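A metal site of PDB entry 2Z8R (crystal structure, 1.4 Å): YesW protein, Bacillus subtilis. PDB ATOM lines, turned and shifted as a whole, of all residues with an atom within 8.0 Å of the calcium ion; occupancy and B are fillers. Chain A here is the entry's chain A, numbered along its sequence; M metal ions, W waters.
N of Glu 379 lies within hydrogen-bond range of O of Gly 369 (2.9 Å). The side-chain carboxylate of Asp 372 is in hydrogen-bond range of the backbone NH of Gly 374 (3.0 Å). OE1 of Glu 379 lies close to N of Leu 371 (3.0 Å). The backbone carbonyl oxygen (O) of Leu 378 sits at hydrogen-bond distance from the guanidinium group (NH2) of Arg 375, 3.0 Å away.
The nearest printed residue that does not touch the calcium ion is Pro 373 (4.2 Å).
The backbone carbonyl oxygen (O) of Gly 377 is bound to the calcium ion, at 2.3 Å. The calcium ion is bound by the backbone carbonyl oxygen (O) of Arg 375, 2.3 Å away. OD1 of Asp 370 binds the calcium ion. The calcium ion is bound by O of Asp 372, 2.4 Å away. Water W1 is bound to the calcium ion (2.4 Å). The side-chain carboxylate (OE2) of Glu 379 is bound to the calcium ion. The calcium ion is bound by the side-chain carboxylate (OE1) of Glu 379 (2.7 Å).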
ATOM      1  N   GLY A 369      20.187   5.118   7.370  1.00  0.00           N
ATOM      2  CA  GLY A 369      18.830   5.618   7.214  1.00  0.00           C
ATOM      3  C   GLY A 369      17.877   4.485   7.454  1.00  0.00           C
ATOM      4  O   GLY A 369      18.282   3.433   7.958  1.00  0.00           O
ATOM      5  N   ASP A 370      16.604   4.688   7.114  1.00  0.00           N
ATOM      6  CA  ASP A 370      15.681   3.571   7.171  1.00  0.00           C
ATOM      7  C   ASP A 370      15.758   2.862   5.825  1.00  0.00           C
ATOM      8  O   ASP A 370      14.997   3.183   4.894  1.00  0.00           O
ATOM      9  CB  ASP A 370      14.263   3.980   7.548  1.00  0.00           C
ATOM     10  CG  ASP A 370      13.422   2.786   7.932  1.00  0.00           C
ATOM     11  OD1 ASP A 370      13.980   1.663   7.922  1.00  0.00           O
ATOM     12  OD2 ASP A 370      12.224   2.956   8.236  1.00  0.00           O
ATOM     13  N   LEU A 371      16.713   1.946   5.713  1.00  0.00           N
ATOM     14  CA  LEU A 371      16.963   1.267   4.454  1.00  0.00           C
ATOM     15  C   LEU A 371      15.981   0.121   4.260  1.00  0.00           C
ATOM     16  O   LEU A 371      15.523  -0.133   3.140  1.00  0.00           O
ATOM     17  CB  LEU A 371      18.417   0.773   4.395  1.00  0.00           C
ATOM     18  CG  LEU A 371      19.504   1.778   4.782  1.00  0.00           C
ATOM     19  CD1 LEU A 371      20.884   1.147   4.578  1.00  0.00           C
ATOM     20  CD2 LEU A 371      19.373   3.090   3.982  1.00  0.00           C
ATOM     21  N   ASP A 372      15.661  -0.574   5.349  1.00  0.00           N
ATOM     22  CA  ASP A 372      14.688  -1.655   5.341  1.00  0.00           C
ATOM     23  C   ASP A 372      13.507  -1.246   6.210  1.00  0.00           C
ATOM     24  O   ASP A 372      13.549  -1.431   7.435  1.00  0.00           O
ATOM     25  CB  ASP A 372      15.285  -2.947   5.868  1.00  0.00           C
ATOM     26  CG  ASP A 372      14.313  -4.117   5.779  1.00  0.00           C
ATOM     27  OD1 ASP A 372      14.749  -5.253   6.069  1.00  0.00           O
ATOM     28  OD2 ASP A 372      13.138  -3.889   5.428  1.00  0.00           O
ATOM     29  N   PRO A 373      12.435  -0.700   5.601  1.00  0.00           N
ATOM     30  CA  PRO A 373      11.291  -0.207   6.358  1.00  0.00           C
ATOM     31  C   PRO A 373      10.444  -1.337   6.960  1.00  0.00           C
ATOM     32  O   PRO A 373       9.578  -1.060   7.768  1.00  0.00           O
ATOM     33  CB  PRO A 373      10.490   0.586   5.330  1.00  0.00           C
ATOM     34  CG  PRO A 373      10.810  -0.051   4.024  1.00  0.00           C
ATOM     35  CD  PRO A 373      12.256  -0.502   4.142  1.00  0.00           C
ATOM     36  N   GLY A 374      10.730  -2.572   6.589  1.00  0.00           N
ATOM     37  CA  GLY A 374      10.030  -3.730   7.167  1.00  0.00           C
ATOM     38  C   GLY A 374      10.693  -4.231   8.443  1.00  0.00           C
ATOM     39  O   GLY A 374      10.167  -5.109   9.133  1.00  0.00           O
ATOM     40  N   ARG A 375      11.853  -3.665   8.760  1.00  0.00           N
ATOM     41  CA  ARG A 375      12.611  -4.076   9.938  1.00  0.00           C
ATOM     42  C   ARG A 375      12.717  -2.872  10.878  1.00  0.00           C
ATOM     43  O   ARG A 375      13.290  -1.859  10.499  1.00  0.00           O
ATOM     44  CB  ARG A 375      14.019  -4.522   9.530  1.00  0.00           C
ATOM     45  CG  ARG A 375      14.757  -5.268  10.647  1.00  0.00           C
ATOM     46  CD  ARG A 375      16.264  -5.182  10.425  1.00  0.00           C
ATOM     47  NE  ARG A 375      16.793  -3.890  10.852  1.00  0.00           N
ATOM     48  CZ  ARG A 375      17.224  -3.621  12.075  1.00  0.00           C
ATOM     49  NH1 ARG A 375      17.214  -4.569  13.024  1.00  0.00           N
ATOM     50  NH2 ARG A 375      17.678  -2.412  12.367  1.00  0.00           N
ATOM     51  N   PRO A 376      12.126  -2.959  12.084  1.00  0.00           N
ATOM     52  CA  PRO A 376      12.222  -1.826  13.014  1.00  0.00           C
ATOM     53  C   PRO A 376      13.661  -1.395  13.280  1.00  0.00           C
ATOM     54  O   PRO A 376      14.547  -2.236  13.497  1.00  0.00           O
ATOM     55  CB  PRO A 376      11.573  -2.352  14.300  1.00  0.00           C
ATOM     56  CG  PRO A 376      10.652  -3.411  13.852  1.00  0.00           C
ATOM     57  CD  PRO A 376      11.287  -4.046  12.635  1.00  0.00           C
ATOM     58  N   GLY A 377      13.861  -0.077  13.257  1.00  0.00           N
ATOM     59  CA  GLY A 377      15.163   0.529  13.489  1.00  0.00           C
ATOM     60  C   GLY A 377      15.766   1.046  12.195  1.00  0.00           C
ATOM     61  O   GLY A 377      15.198   0.886  11.120  1.00  0.00           O
ATOM     62  N   LEU A 378      16.926   1.683  12.319  1.00  0.00           N
ATOM     63  CA  LEU A 378      17.682   2.115  11.154  1.00  0.00           C
ATOM     64  C   LEU A 378      18.679   1.029  10.763  1.00  0.00           C
ATOM     65  O   LEU A 378      18.977   0.109  11.532  1.00  0.00           O
ATOM     66  CB  LEU A 378      18.411   3.432  11.446  1.00  0.00           C
ATOM     67  CG  LEU A 378      17.534   4.600  11.890  1.00  0.00           C
ATOM     68  CD1 LEU A 378      18.390   5.829  12.140  1.00  0.00           C
ATOM     69  CD2 LEU A 378      16.463   4.894  10.827  1.00  0.00           C
ATOM     70  N   GLU A 379      19.187   1.168   9.541  1.00  0.00           N
ATOM     71  CA  GLU A 379      20.151   0.231   9.012  1.00  0.00           C
ATOM     72  C   GLU A 379      21.339   1.002   8.469  1.00  0.00           C
ATOM     73  O   GLU A 379      21.225   2.182   8.114  1.00  0.00           O
ATOM     74  CB  GLU A 379      19.508  -0.645   7.927  1.00  0.00           C
ATOM     75  CG  GLU A 379      18.461  -1.624   8.465  1.00  0.00           C
ATOM     76  CD  GLU A 379      17.070  -1.018   8.681  1.00  0.00           C
ATOM     77  OE1 GLU A 379      16.681  -0.037   8.002  1.00  0.00           O
ATOM     78  OE2 GLU A 379      16.348  -1.556   9.543  1.00  0.00           O
ATOM     79  N   PHE A 395      25.553  -4.871   5.604  1.00  0.00           N
ATOM     80  CA  PHE A 395      24.256  -4.255   5.826  1.00  0.00           C
ATOM     81  C   PHE A 395      23.849  -4.680   7.236  1.00  0.00           C
ATOM     82  O   PHE A 395      23.689  -5.884   7.521  1.00  0.00           O
ATOM     83  CB  PHE A 395      23.262  -4.788   4.785  1.00  0.00           C
ATOM     84  CG  PHE A 395      21.943  -4.055   4.744  1.00  0.00           C
ATOM     85  CD1 PHE A 395      21.690  -3.070   3.783  1.00  0.00           C
ATOM     86  CD2 PHE A 395      20.931  -4.367   5.639  1.00  0.00           C
ATOM     87  CE1 PHE A 395      20.450  -2.423   3.734  1.00  0.00           C
ATOM     88  CE2 PHE A 395      19.704  -3.722   5.596  1.00  0.00           C
ATOM     89  CZ  PHE A 395      19.460  -2.748   4.645  1.00  0.00           C
ATOM     90  N   LEU A 404      23.059  -8.021   9.224  1.00  0.00           N
ATOM     91  CA  LEU A 404      21.848  -8.583   8.654  1.00  0.00           C
ATOM     92  C   LEU A 404      22.180  -9.419   7.418  1.00  0.00           C
ATOM     93  O   LEU A 404      21.681 -10.528   7.239  1.00  0.00           O
ATOM     94  CB  LEU A 404      20.838  -7.470   8.346  1.00  0.00           C
ATOM     95  CG  LEU A 404      20.413  -6.624   9.546  1.00  0.00           C
ATOM     96  CD1 LEU A 404      19.708  -5.329   9.122  1.00  0.00           C
ATOM     97  CD2 LEU A 404      19.542  -7.428  10.514  1.00  0.00           C
ATOM     98  N   SER A 565      15.479  10.403   8.320  1.00  0.00           N
ATOM     99  CA  SER A 565      15.299   9.515   9.481  1.00  0.00           C
ATOM    100  C   SER A 565      14.227   8.456   9.263  1.00  0.00           C
ATOM    101  O   SER A 565      14.200   7.432   9.951  1.00  0.00           O
ATOM    102  CB  SER A 565      14.947  10.331  10.733  1.00  0.00           C
ATOM    103  OG  SER A 565      13.661  10.934  10.628  1.00  0.00           O
ATOM    104  N   PHE A 567      11.675   6.252   6.219  1.00  0.00           N
ATOM    105  CA  PHE A 567      11.715   5.726   4.866  1.00  0.00           C
ATOM    106  C   PHE A 567      10.929   6.645   3.936  1.00  0.00           C
ATOM    107  O   PHE A 567       9.699   6.759   4.005  1.00  0.00           O
ATOM    108  CB  PHE A 567      11.168   4.303   4.786  1.00  0.00           C
ATOM    109  CG  PHE A 567      11.056   3.792   3.358  1.00  0.00           C
ATOM    110  CD1 PHE A 567      12.193   3.545   2.607  1.00  0.00           C
ATOM    111  CD2 PHE A 567       9.813   3.586   2.777  1.00  0.00           C
ATOM    112  CE1 PHE A 567      12.105   3.097   1.277  1.00  0.00           C
ATOM    113  CE2 PHE A 567       9.709   3.148   1.452  1.00  0.00           C
ATOM    114  CZ  PHE A 567      10.851   2.887   0.703  1.00  0.00           C
HETATM  115 CA    CA M   1      14.317  -0.185   9.295  1.00  0.00          CA
HETATM  116  O   HOH W   1      12.117   0.706   9.881  1.00  0.00           O
